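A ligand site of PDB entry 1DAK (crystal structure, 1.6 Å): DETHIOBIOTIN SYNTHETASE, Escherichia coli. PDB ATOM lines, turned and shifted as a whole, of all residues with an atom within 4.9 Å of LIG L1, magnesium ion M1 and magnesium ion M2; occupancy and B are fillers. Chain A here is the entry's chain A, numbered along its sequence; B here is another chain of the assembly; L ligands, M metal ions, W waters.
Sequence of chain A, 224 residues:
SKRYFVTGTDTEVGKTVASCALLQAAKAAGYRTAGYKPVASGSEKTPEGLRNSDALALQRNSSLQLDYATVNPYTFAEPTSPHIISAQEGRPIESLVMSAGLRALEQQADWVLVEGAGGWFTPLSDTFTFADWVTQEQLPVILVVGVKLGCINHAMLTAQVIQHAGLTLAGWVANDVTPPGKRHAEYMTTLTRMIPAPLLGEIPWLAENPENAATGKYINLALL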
ATOM      1  N   ASP A  10      36.428   3.894 -10.478  1.00  0.00           N
ATOM      2  CA  ASP A  10      35.413   4.636 -11.224  1.00  0.00           C
ATOM      3  C   ASP A  10      34.530   3.622 -11.943  1.00  0.00           C
ATOM      4  O   ASP A  10      34.717   2.408 -11.782  1.00  0.00           O
ATOM      5  CB  ASP A  10      36.117   5.561 -12.218  1.00  0.00           C
ATOM      6  CG  ASP A  10      35.255   6.623 -12.865  1.00  0.00           C
ATOM      7  OD1 ASP A  10      34.053   6.713 -12.557  1.00  0.00           O
ATOM      8  OD2 ASP A  10      35.785   7.379 -13.702  1.00  0.00           O
ATOM      9  N   THR A  11      33.593   4.104 -12.754  1.00  0.00           N
ATOM     10  CA  THR A  11      32.886   3.202 -13.670  1.00  0.00           C
ATOM     11  C   THR A  11      33.850   3.066 -14.854  1.00  0.00           C
ATOM     12  O   THR A  11      34.766   3.857 -15.021  1.00  0.00           O
ATOM     13  CB  THR A  11      31.520   3.733 -14.113  1.00  0.00           C
ATOM     14  OG1 THR A  11      30.814   2.748 -14.888  1.00  0.00           O
ATOM     15  CG2 THR A  11      31.666   4.988 -14.956  1.00  0.00           C
ATOM     16  N   GLU A  12      33.748   2.031 -15.653  1.00  0.00           N
ATOM     17  CA  GLU A  12      34.569   1.769 -16.829  1.00  0.00           C
ATOM     18  C   GLU A  12      36.051   1.580 -16.559  1.00  0.00           C
ATOM     19  O   GLU A  12      36.869   2.060 -17.335  1.00  0.00           O
ATOM     20  CB  GLU A  12      34.338   2.868 -17.880  1.00  0.00           C
ATOM     21  CG  GLU A  12      34.636   2.409 -19.297  1.00  0.00           C
ATOM     22  CD  GLU A  12      33.521   1.618 -19.946  1.00  0.00           C
ATOM     23  OE1 GLU A  12      32.375   1.643 -19.455  1.00  0.00           O
ATOM     24  OE2 GLU A  12      33.775   0.978 -20.991  1.00  0.00           O
ATOM     25  N   LYS A  15      35.890  -3.485 -13.344  1.00  0.00           N
ATOM     26  CA  LYS A  15      35.270  -4.271 -12.279  1.00  0.00           C
ATOM     27  C   LYS A  15      34.773  -5.598 -12.855  1.00  0.00           C
ATOM     28  O   LYS A  15      34.990  -6.626 -12.245  1.00  0.00           O
ATOM     29  CB  LYS A  15      34.094  -3.600 -11.558  1.00  0.00           C
ATOM     30  CG  LYS A  15      34.441  -2.355 -10.765  1.00  0.00           C
ATOM     31  CD  LYS A  15      33.222  -1.820 -10.013  1.00  0.00           C
ATOM     32  CE  LYS A  15      32.085  -1.412 -10.928  1.00  0.00           C
ATOM     33  NZ  LYS A  15      32.415  -0.176 -11.697  1.00  0.00           N
ATOM     34  N   THR A  16      34.092  -5.575 -13.993  1.00  0.00           N
ATOM     35  CA  THR A  16      33.461  -6.767 -14.553  1.00  0.00           C
ATOM     36  C   THR A  16      34.538  -7.715 -15.063  1.00  0.00           C
ATOM     37  O   THR A  16      34.499  -8.886 -14.689  1.00  0.00           O
ATOM     38  CB  THR A  16      32.417  -6.441 -15.625  1.00  0.00           C
ATOM     39  OG1 THR A  16      31.387  -5.631 -15.022  1.00  0.00           O
ATOM     40  CG2 THR A  16      31.782  -7.669 -16.245  1.00  0.00           C
ATOM     41  N   LYS A  37      25.138  -9.209  -9.302  1.00  0.00           N
ATOM     42  CA  LYS A  37      25.145  -7.777  -9.691  1.00  0.00           C
ATOM     43  C   LYS A  37      23.746  -7.292  -9.323  1.00  0.00           C
ATOM     44  O   LYS A  37      22.855  -7.324 -10.176  1.00  0.00           O
ATOM     45  CB  LYS A  37      25.396  -7.653 -11.187  1.00  0.00           C
ATOM     46  CG  LYS A  37      25.288  -6.250 -11.788  1.00  0.00           C
ATOM     47  CD  LYS A  37      26.597  -5.481 -11.765  1.00  0.00           C
ATOM     48  CE  LYS A  37      26.421  -4.111 -12.408  1.00  0.00           C
ATOM     49  NZ  LYS A  37      27.710  -3.336 -12.435  1.00  0.00           N
ATOM     50  N   VAL A  39      22.274  -4.470  -8.698  1.00  0.00           N
ATOM     51  CA  VAL A  39      21.720  -3.309  -9.398  1.00  0.00           C
ATOM     52  C   VAL A  39      22.532  -3.049 -10.661  1.00  0.00           C
ATOM     53  O   VAL A  39      23.758  -2.949 -10.611  1.00  0.00           O
ATOM     54  CB  VAL A  39      21.766  -2.076  -8.473  1.00  0.00           C
ATOM     55  CG1 VAL A  39      21.323  -0.827  -9.241  1.00  0.00           C
ATOM     56  CG2 VAL A  39      20.894  -2.241  -7.242  1.00  0.00           C
ATOM     57  N   ALA A  40      21.840  -2.935 -11.801  1.00  0.00           N
ATOM     58  CA  ALA A  40      22.511  -2.682 -13.067  1.00  0.00           C
ATOM     59  C   ALA A  40      21.707  -1.684 -13.912  1.00  0.00           C
ATOM     60  O   ALA A  40      20.486  -1.762 -13.952  1.00  0.00           O
ATOM     61  CB  ALA A  40      22.677  -3.988 -13.836  1.00  0.00           C
ATOM     62  N   SER A  41      22.402  -0.768 -14.556  1.00  0.00           N
ATOM     63  CA  SER A  41      21.790   0.217 -15.445  1.00  0.00           C
ATOM     64  C   SER A  41      22.549   0.148 -16.766  1.00  0.00           C
ATOM     65  O   SER A  41      23.778   0.043 -16.743  1.00  0.00           O
ATOM     66  CB  SER A  41      21.816   1.621 -14.863  1.00  0.00           C
ATOM     67  OG  SER A  41      23.126   2.034 -14.485  1.00  0.00           O
ATOM     68  N   ASN A  52      21.409  -7.112 -18.719  1.00  0.00           N
ATOM     69  CA  ASN A  52      22.621  -6.297 -18.609  1.00  0.00           C
ATOM     70  C   ASN A  52      23.858  -7.135 -18.906  1.00  0.00           C
ATOM     71  O   ASN A  52      23.933  -8.250 -18.399  1.00  0.00           O
ATOM     72  CB  ASN A  52      22.700  -5.706 -17.204  1.00  0.00           C
ATOM     73  CG  ASN A  52      24.029  -5.080 -16.858  1.00  0.00           C
ATOM     74  OD1 ASN A  52      24.929  -5.716 -16.286  1.00  0.00           O
ATOM     75  ND2 ASN A  52      24.162  -3.819 -17.202  1.00  0.00           N
ATOM     76  N   ASP A  54      27.046  -6.844 -17.838  1.00  0.00           N
ATOM     77  CA  ASP A  54      27.848  -7.193 -16.672  1.00  0.00           C
ATOM     78  C   ASP A  54      27.252  -8.429 -16.011  1.00  0.00           C
ATOM     79  O   ASP A  54      27.935  -9.405 -15.700  1.00  0.00           O
ATOM     80  CB  ASP A  54      27.883  -6.100 -15.595  1.00  0.00           C
ATOM     81  CG  ASP A  54      28.662  -4.858 -15.932  1.00  0.00           C
ATOM     82  OD1 ASP A  54      29.036  -4.659 -17.106  1.00  0.00           O
ATOM     83  OD2 ASP A  54      28.942  -4.095 -14.985  1.00  0.00           O
ATOM     84  N   PRO A  79      21.750   3.672 -19.164  1.00  0.00           N
ATOM     85  CA  PRO A  79      23.042   3.692 -18.511  1.00  0.00           C
ATOM     86  C   PRO A  79      23.367   4.985 -17.789  1.00  0.00           C
ATOM     87  O   PRO A  79      24.312   5.711 -18.135  1.00  0.00           O
ATOM     88  CB  PRO A  79      24.011   3.417 -19.653  1.00  0.00           C
ATOM     89  CG  PRO A  79      23.361   4.034 -20.848  1.00  0.00           C
ATOM     90  CD  PRO A  79      21.875   3.883 -20.634  1.00  0.00           C
ATOM     91  N   THR A  80      22.684   5.231 -16.680  1.00  0.00           N
ATOM     92  CA  THR A  80      22.891   6.414 -15.860  1.00  0.00           C
ATOM     93  C   THR A  80      23.036   6.010 -14.400  1.00  0.00           C
ATOM     94  O   THR A  80      23.114   4.800 -14.112  1.00  0.00           O
ATOM     95  CB  THR A  80      21.723   7.412 -16.043  1.00  0.00           C
ATOM     96  OG1 THR A  80      22.052   8.647 -15.381  1.00  0.00           O
ATOM     97  CG2 THR A  80      20.446   6.851 -15.458  1.00  0.00           C
ATOM     98  N   SER A  81      23.068   6.932 -13.451  1.00  0.00           N
ATOM     99  CA  SER A  81      23.137   6.530 -12.033  1.00  0.00           C
ATOM    100  C   SER A  81      21.837   5.817 -11.667  1.00  0.00           C
ATOM    101  O   SER A  81      20.734   6.270 -12.012  1.00  0.00           O
ATOM    102  CB  SER A  81      23.333   7.777 -11.175  1.00  0.00           C
ATOM    103  OG  SER A  81      23.548   7.445  -9.824  1.00  0.00           O
ATOM    104  N   PRO A  82      21.929   4.699 -10.970  1.00  0.00           N
ATOM    105  CA  PRO A  82      20.752   3.913 -10.599  1.00  0.00           C
ATOM    106  C   PRO A  82      19.657   4.728  -9.958  1.00  0.00           C
ATOM    107  O   PRO A  82      18.469   4.582 -10.306  1.00  0.00           O
ATOM    108  CB  PRO A  82      21.291   2.818  -9.690  1.00  0.00           C
ATOM    109  CG  PRO A  82      22.712   2.652 -10.122  1.00  0.00           C
ATOM    110  CD  PRO A  82      23.174   4.034 -10.539  1.00  0.00           C
ATOM    111  N   GLU A 115      29.303  -7.609  -7.546  1.00  0.00           N
ATOM    112  CA  GLU A 115      29.870  -6.467  -8.267  1.00  0.00           C
ATOM    113  C   GLU A 115      28.978  -5.252  -8.015  1.00  0.00           C
ATOM    114  O   GLU A 115      27.762  -5.361  -8.165  1.00  0.00           O
ATOM    115  CB  GLU A 115      30.017  -6.695  -9.770  1.00  0.00           C
ATOM    116  CG  GLU A 115      30.702  -5.526 -10.479  1.00  0.00           C
ATOM    117  CD  GLU A 115      30.645  -5.459 -11.982  1.00  0.00           C
ATOM    118  OE1 GLU A 115      30.448  -6.490 -12.653  1.00  0.00           O
ATOM    119  OE2 GLU A 115      30.820  -4.355 -12.572  1.00  0.00           O
ATOM    120  N   GLY A 116      29.611  -4.155  -7.624  1.00  0.00           N
ATOM    121  CA  GLY A 116      28.846  -2.906  -7.420  1.00  0.00           C
ATOM    122  C   GLY A 116      28.545  -2.268  -8.777  1.00  0.00           C
ATOM    123  O   GLY A 116      28.664  -2.879  -9.826  1.00  0.00           O
ATOM    124  N   ALA A 117      28.054  -1.037  -8.726  1.00  0.00           N
ATOM    125  CA  ALA A 117      27.773  -0.282  -9.943  1.00  0.00           C
ATOM    126  C   ALA A 117      28.500   1.057  -9.792  1.00  0.00           C
ATOM    127  O   ALA A 117      28.466   1.659  -8.711  1.00  0.00           O
ATOM    128  CB  ALA A 117      26.291  -0.106 -10.194  1.00  0.00           C
ATOM    129  N   GLY A 118      29.223   1.437 -10.829  1.00  0.00           N
ATOM    130  CA  GLY A 118      30.042   2.651 -10.765  1.00  0.00           C
ATOM    131  C   GLY A 118      31.092   2.482  -9.675  1.00  0.00           C
ATOM    132  O   GLY A 118      31.677   1.393  -9.505  1.00  0.00           O
ATOM    133  N   THR A 122      28.111   5.385  -5.468  1.00  0.00           N
ATOM    134  CA  THR A 122      26.969   5.460  -6.389  1.00  0.00           C
ATOM    135  C   THR A 122      25.641   5.444  -5.652  1.00  0.00           C
ATOM    136  O   THR A 122      25.322   4.484  -4.947  1.00  0.00           O
ATOM    137  CB  THR A 122      27.050   4.218  -7.311  1.00  0.00           C
ATOM    138  OG1 THR A 122      28.239   4.347  -8.092  1.00  0.00           O
ATOM    139  CG2 THR A 122      25.844   4.149  -8.221  1.00  0.00           C
ATOM    140  N   PRO A 123      24.793   6.449  -5.887  1.00  0.00           N
ATOM    141  CA  PRO A 123      23.498   6.512  -5.211  1.00  0.00           C
ATOM    142  C   PRO A 123      22.497   5.495  -5.733  1.00  0.00           C
ATOM    143  O   PRO A 123      22.439   5.262  -6.942  1.00  0.00           O
ATOM    144  CB  PRO A 123      23.007   7.922  -5.503  1.00  0.00           C
ATOM    145  CG  PRO A 123      24.261   8.705  -5.831  1.00  0.00           C
ATOM    146  CD  PRO A 123      25.092   7.698  -6.627  1.00  0.00           C
ATOM    147  N   LYS B 148      30.211  14.420 -15.519  1.00  0.00           N
ATOM    148  CA  LYS B 148      30.224  13.240 -16.373  1.00  0.00           C
ATOM    149  C   LYS B 148      29.913  12.013 -15.524  1.00  0.00           C
ATOM    150  O   LYS B 148      29.879  12.086 -14.296  1.00  0.00           O
ATOM    151  CB  LYS B 148      31.566  13.080 -17.067  1.00  0.00           C
ATOM    152  CG  LYS B 148      32.748  12.887 -16.134  1.00  0.00           C
ATOM    153  CD  LYS B 148      34.035  12.899 -16.941  1.00  0.00           C
ATOM    154  CE  LYS B 148      35.252  12.757 -16.058  1.00  0.00           C
ATOM    155  NZ  LYS B 148      36.519  12.585 -16.833  1.00  0.00           N
ATOM    156  N   LEU B 149      29.643  10.886 -16.197  1.00  0.00           N
ATOM    157  CA  LEU B 149      29.328   9.665 -15.468  1.00  0.00           C
ATOM    158  C   LEU B 149      30.469   9.306 -14.534  1.00  0.00           C
ATOM    159  O   LEU B 149      31.622   9.261 -14.994  1.00  0.00           O
ATOM    160  CB  LEU B 149      29.080   8.548 -16.480  1.00  0.00           C
ATOM    161  CG  LEU B 149      28.247   7.355 -16.025  1.00  0.00           C
ATOM    162  CD1 LEU B 149      26.773   7.734 -15.878  1.00  0.00           C
ATOM    163  CD2 LEU B 149      28.403   6.208 -17.026  1.00  0.00           C
ATOM    164  N   GLY B 150      30.172   9.077 -13.268  1.00  0.00           N
ATOM    165  CA  GLY B 150      31.182   8.742 -12.277  1.00  0.00           C
ATOM    166  C   GLY B 150      31.579   9.941 -11.423  1.00  0.00           C
ATOM    167  O   GLY B 150      32.219   9.781 -10.384  1.00  0.00           O
ATOM    168  N   CYS B 151      31.113  11.153 -11.771  1.00  0.00           N
ATOM    169  CA  CYS B 151      31.492  12.329 -11.006  1.00  0.00           C
ATOM    170  C   CYS B 151      30.851  12.425  -9.633  1.00  0.00           C
ATOM    171  O   CYS B 151      31.430  13.053  -8.737  1.00  0.00           O
ATOM    172  CB  CYS B 151      31.275  13.617 -11.809  1.00  0.00           C
ATOM    173  SG  CYS B 151      29.565  14.187 -11.921  1.00  0.00           S
ATOM    174  N   ILE B 152      29.694  11.773  -9.424  1.00  0.00           N
ATOM    175  CA  ILE B 152      29.050  11.818  -8.111  1.00  0.00           C
ATOM    176  C   ILE B 152      29.948  11.139  -7.078  1.00  0.00           C
ATOM    177  O   ILE B 152      30.300  11.687  -6.036  1.00  0.00           O
ATOM    178  CB  ILE B 152      27.649  11.201  -8.128  1.00  0.00           C
ATOM    179  CG1 ILE B 152      26.691  12.014  -9.014  1.00  0.00           C
ATOM    180  CG2 ILE B 152      27.076  11.209  -6.723  1.00  0.00           C
ATOM    181  CD1 ILE B 152      25.425  11.291  -9.417  1.00  0.00           C
ATOM    182  N   ASN B 153      30.375   9.915  -7.401  1.00  0.00           N
ATOM    183  CA  ASN B 153      31.274   9.156  -6.538  1.00  0.00           C
ATOM    184  C   ASN B 153      32.570   9.935  -6.275  1.00  0.00           C
ATOM    185  O   ASN B 153      32.945  10.068  -5.127  1.00  0.00           O
ATOM    186  CB  ASN B 153      31.623   7.817  -7.211  1.00  0.00           C
ATOM    187  CG  ASN B 153      32.676   7.027  -6.474  1.00  0.00           C
ATOM    188  OD1 ASN B 153      32.585   6.800  -5.262  1.00  0.00           O
ATOM    189  ND2 ASN B 153      33.720   6.598  -7.211  1.00  0.00           N
ATOM    190  N   TYR B 187      21.846  15.284 -12.543  1.00  0.00           N
ATOM    191  CA  TYR B 187      23.198  15.171 -11.997  1.00  0.00           C
ATOM    192  C   TYR B 187      23.515  16.415 -11.175  1.00  0.00           C
ATOM    193  O   TYR B 187      23.978  16.347 -10.032  1.00  0.00           O
ATOM    194  CB  TYR B 187      24.206  14.968 -13.139  1.00  0.00           C
ATOM    195  CG  TYR B 187      24.746  13.542 -13.096  1.00  0.00           C
ATOM    196  CD1 TYR B 187      23.978  12.474 -13.522  1.00  0.00           C
ATOM    197  CD2 TYR B 187      26.013  13.290 -12.580  1.00  0.00           C
ATOM    198  CE1 TYR B 187      24.456  11.173 -13.472  1.00  0.00           C
ATOM    199  CE2 TYR B 187      26.496  11.997 -12.510  1.00  0.00           C
ATOM    200  CZ  TYR B 187      25.707  10.948 -12.947  1.00  0.00           C
ATOM    201  OH  TYR B 187      26.218   9.671 -12.867  1.00  0.00           O
HETATM  202  C1  LIG L   1      27.387   7.324 -10.475  1.00  0.00           C
HETATM  203  C2  LIG L   1      28.346   8.532 -10.316  1.00  0.00           C
HETATM  204  O1  LIG L   1      28.244   9.486 -11.122  1.00  0.00           O
HETATM  205  O2  LIG L   1      29.260   8.382  -9.470  1.00  0.00           O
HETATM  206  C3  LIG L   1      27.801   6.596 -11.775  1.00  0.00           C
HETATM  207  C4  LIG L   1      27.002   5.309 -11.988  1.00  0.00           C
HETATM  208  C5  LIG L   1      27.477   4.415 -13.165  1.00  0.00           C
HETATM  209  C6  LIG L   1      26.577   3.140 -13.261  1.00  0.00           C
HETATM  210  C7  LIG L   1      27.002   2.182 -14.328  1.00  0.00           C
HETATM  211  C8  LIG L   1      27.470   2.622 -15.732  1.00  0.00           C
HETATM  212  C9  LIG L   1      26.247   3.149 -16.511  1.00  0.00           C
HETATM  213  N1  LIG L   1      25.841   0.939 -14.251  1.00  0.00           N
HETATM  214  N2  LIG L   1      27.888   1.357 -16.465  1.00  0.00           N
HETATM  215  C10 LIG L   1      26.376  -0.335 -14.000  1.00  0.00           C
HETATM  216  O3  LIG L   1      25.461  -1.233 -13.941  1.00  0.00           O
HETATM  217  O4  LIG L   1      30.139  -1.696 -13.535  1.00  0.00           O
HETATM  218  P1  LIG L   1      29.618  -0.394 -13.866  1.00  0.00           P
HETATM  219  O5  LIG L   1      27.914  -0.620 -13.237  1.00  0.00           O
HETATM  220  O6  LIG L   1      29.425  -0.311 -15.333  1.00  0.00           O
HETATM  221  O7  LIG L   1      30.441   0.758 -13.250  1.00  0.00           O
HETATM  222  P1  LG2 L   2      33.560  -1.523 -15.061  1.00  0.00           P
HETATM  223  O1  LG2 L   2      34.318  -0.871 -14.000  1.00  0.00           O
HETATM  224  O2  LG2 L   2      32.500  -0.740 -15.759  1.00  0.00           O
HETATM  225  O3  LG2 L   2      32.854  -2.926 -14.780  1.00  0.00           O
HETATM  226  P2  LG2 L   2      34.510  -3.325 -17.353  1.00  0.00           P
HETATM  227  O4  LG2 L   2      33.127  -3.440 -17.938  1.00  0.00           O
HETATM  228  O5  LG2 L   2      35.078  -4.579 -16.792  1.00  0.00           O
HETATM  229  O6  LG2 L   2      34.605  -2.030 -16.238  1.00  0.00           O
HETATM  230  O7  LG2 L   2      35.585  -2.710 -18.465  1.00  0.00           O
HETATM  231  C1  LG2 L   2      35.262  -1.396 -19.071  1.00  0.00           C
HETATM  232  C2  LG2 L   2      35.580  -1.495 -20.562  1.00  0.00           C
HETATM  233  O8  LG2 L   2      36.983  -1.729 -20.703  1.00  0.00           O
HETATM  234  C3  LG2 L   2      34.895  -2.691 -21.234  1.00  0.00           C
HETATM  235  O9  LG2 L   2      34.556  -2.422 -22.616  1.00  0.00           O
HETATM  236  C4  LG2 L   2      35.910  -3.831 -21.142  1.00  0.00           C
HETATM  237  O10 LG2 L   2      35.699  -4.819 -22.175  1.00  0.00           O
HETATM  238  C5  LG2 L   2      37.229  -3.057 -21.289  1.00  0.00           C
HETATM  239  N1  LG2 L   2      38.321  -3.788 -20.521  1.00  0.00           N
HETATM  240  C6  LG2 L   2      38.323  -3.938 -19.198  1.00  0.00           C
HETATM  241  N2  LG2 L   2      39.479  -4.467 -18.822  1.00  0.00           N
HETATM  242  C7  LG2 L   2      40.180  -4.797 -19.900  1.00  0.00           C
HETATM  243  C8  LG2 L   2      41.436  -5.371 -20.060  1.00  0.00           C
HETATM  244  N3  LG2 L   2      42.199  -5.752 -19.025  1.00  0.00           N
HETATM  245  N4  LG2 L   2      41.965  -5.286 -21.298  1.00  0.00           N
HETATM  246  C9  LG2 L   2      41.325  -4.679 -22.303  1.00  0.00           C
HETATM  247  N5  LG2 L   2      40.038  -4.306 -22.221  1.00  0.00           N
HETATM  248  C10 LG2 L   2      39.501  -4.249 -20.975  1.00  0.00           C
HETATM  249 MG    MG M   1      30.934  -3.479 -14.532  1.00  0.00          MG
HETATM  250 MG    MG M   2      30.745  -0.754 -16.914  1.00  0.00          MG
HETATM  251  O   HOH W   1      26.737  -2.384 -16.384  1.00  0.00           O
HETATM  252  O   HOH W   2      26.202  -0.258 -17.937  1.00  0.00           O
HETATM  253  O   HOH W   3      31.802  -0.980 -18.805  1.00  0.00           O
HETATM  254  O   HOH W   4      29.078  -0.765 -18.187  1.00  0.00           O
HETATM  255  O   HOH W   5      30.843  -2.806 -16.694  1.00  0.00           O
HETATM  256  O   HOH W   6      30.734   5.989  -9.851  1.00  0.00           O
HETATM  257  O   HOH W   7      30.861   1.431 -17.450  1.00  0.00           O
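The backbone NH (N) of Cys 151 of chain B lies within hydrogen-bond range of an oxygen (O1) of LIG L1 (3.4 Å).
The side-chain amino group of Lys 37 is in hydrogen-bond range of an oxygen (O5) of LIG L1, 2.8 Å away.
O2 of LIG L1 is in hydrogen-bond range of N of Asn 153 of chain B (2.8 Å).
An oxygen (O5) of LG2 L2 sits at hydrogen-bond distance from the backbone NH of Thr 16 (3.1 Å).
An oxygen (O7) of LIG L1 lies within hydrogen-bond range of the backbone NH (N) of Gly 118 (2.8 Å).
O7 of LIG L1 is in salt-bridge range of NZ of Lys 15, at 2.7 Å.
N of Ser 41 sits at hydrogen-bond distance from O3 of LIG L1 (3.2 Å).
An oxygen (O1) of LG2 L2 is in hydrogen-bond range of the backbone NH of Lys 15 (3.1 Å).
O1 of LIG L1 is in hydrogen-bond range of N of Ile 152 of chain B.
The backbone carbonyl oxygen (O) of Ser 41 is in hydrogen-bond range of a nitrogen (N1) of LIG L1, 3.4 Å away.
The backbone NH (N) of Glu 12 sits at hydrogen-bond distance from an oxygen (O1) of LG2 L2.
OG1 of Thr 11 is in hydrogen-bond range of O7 of LIG L1 (2.6 Å).
The side-chain hydroxyl (OG) of Ser 41 is in hydrogen-bond range of a nitrogen (N1) of LIG L1 (2.9 Å).
The backbone NH of Gly 150 of chain B is in hydrogen-bond range of an oxygen (O1) of LIG L1 (2.9 Å).
O1 of LIG L1 lies within hydrogen-bond range of OH of Tyr 187 of chain B (2.7 Å).
NZ of Lys 15 lies within salt-bridge range of O1 of LG2 L2 (3.1 Å).
The side-chain hydroxyl (OG) of Ser 41 lies within hydrogen-bond range of the backbone carbonyl oxygen (O) of Thr 80.
The side-chain hydroxyl (OG1) of Thr 122 is in hydrogen-bond range of the backbone carbonyl oxygen (O) of Ala 117, at 2.8 Å.
The side-chain sulfur of Cys 151 of chain B lies within hydrogen-bond range of the backbone carbonyl oxygen of Lys 148 of chain B, 3.2 Å away.
The side-chain carboxylate (OE2) of Glu 115 lies close to the side-chain amino group (NZ) of Lys 37, at 3.3 Å.
The side-chain amide oxygen (OD1) of Asn 52 lies within hydrogen-bond range of the backbone NH (N) of Asp 54.
O of Gly 118 sits at hydrogen-bond distance from NZ of Lys 15 (2.8 Å).
The backbone carbonyl oxygen of Gly 116 is in hydrogen-bond range of the side-chain amino group of Lys 37 (2.8 Å).
The side-chain amino group of Lys 15 is in hydrogen-bond range of the backbone carbonyl oxygen of Asp 10 (3.5 Å).
CA of Ala 40 touches O3 of LIG L1, at 3.4 Å.
O of Pro 79 touches C9 of LIG L1, at 3.6 Å.
Thr 80 touches LIG L1 (O to C6, 3.9 Å).
Ser 81 touches LIG L1.
CA of Ala 117 touches O5 of LIG L1, at 3.3 Å.
OG1 of Thr 122 touches C1 of LIG L1, 3.9 Å away.
Leu 149 of chain B touches LIG L1 (CD2 to C9, 3.8 Å).
The nearest printed residue that does not touch LIG L1 is Val 39 (4.1 Å).
Residues that only touch magnesium ion M1: Lys 37.
Of the 28 residues printed, 4 come within 4 Å of magnesium ion M1.
Glu 12 touches magnesium ion M2.
Of the 28 residues printed, 1 comes within 4 Å of magnesium ion M2.
The nearest printed residue that does not touch magnesium ion M2 is Thr 11 (4.05 Å).
An oxygen (O3) of LG2 L2 binds magnesium ion M1.
Magnesium ion M1 is bound by the side-chain carboxylate (OD2) of Asp 54 (2.1 Å).
OE2 of Glu 115 binds magnesium ion M1, 2.1 Å away.
O4 of LIG L1 binds magnesium ion M1 (2.2 Å).
OG1 of Thr 16 is bound to magnesium ion M1, 2.3 Å away.
Magnesium ion M1 is bound by water W5 (2.3 Å).
Magnesium ion M1 has six donor atoms within binding distance.
Magnesium ion M2 is bound by water W5.
Magnesium ion M2 is bound by water W4, at 2.1 Å.
O2 of LG2 L2 is bound to magnesium ion M2 (2.1 Å).
Magnesium ion M2 is bound by an oxygen (O6) of LIG L1.
Magnesium ion M2 is bound by water W3, 2.2 Å away.
Magnesium ion M2 is bound by water W7 (2.3 Å).
Water W5 bridges the side-chain carboxylate of Asp 54 (2.6 Å) and an oxygen (O4) of LG2 L2 (2.7 Å).
Water W7 lies within hydrogen-bond range of the side-chain carboxylate of Glu 12 (2.5 Å), the side-chain hydroxyl of Thr 11 (2.9 Å) and a nitrogen (N2) of LIG L1 (3.1 Å).
Water W3 lies within hydrogen-bond range of the side-chain carboxylate (OE1) of Glu 12 and an oxygen (O4) of LG2 L2.
Water W2 lies within hydrogen-bond range of O of Ser 41 (2.7 Å) and N2 of LIG L1 (2.8 Å).
Water W6 bridges an oxygen (O2) of LIG L1 and the side-chain hydroxyl (OG1) of Thr 122.
Water W1 lies within hydrogen-bond range of an oxygen (O3) of LIG L1 (3.0 Å), the side-chain amide nitrogen (ND2) of Asn 52 (3.1 Å) and the side-chain carboxylate (OD1) of Asp 54 (3.3 Å).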
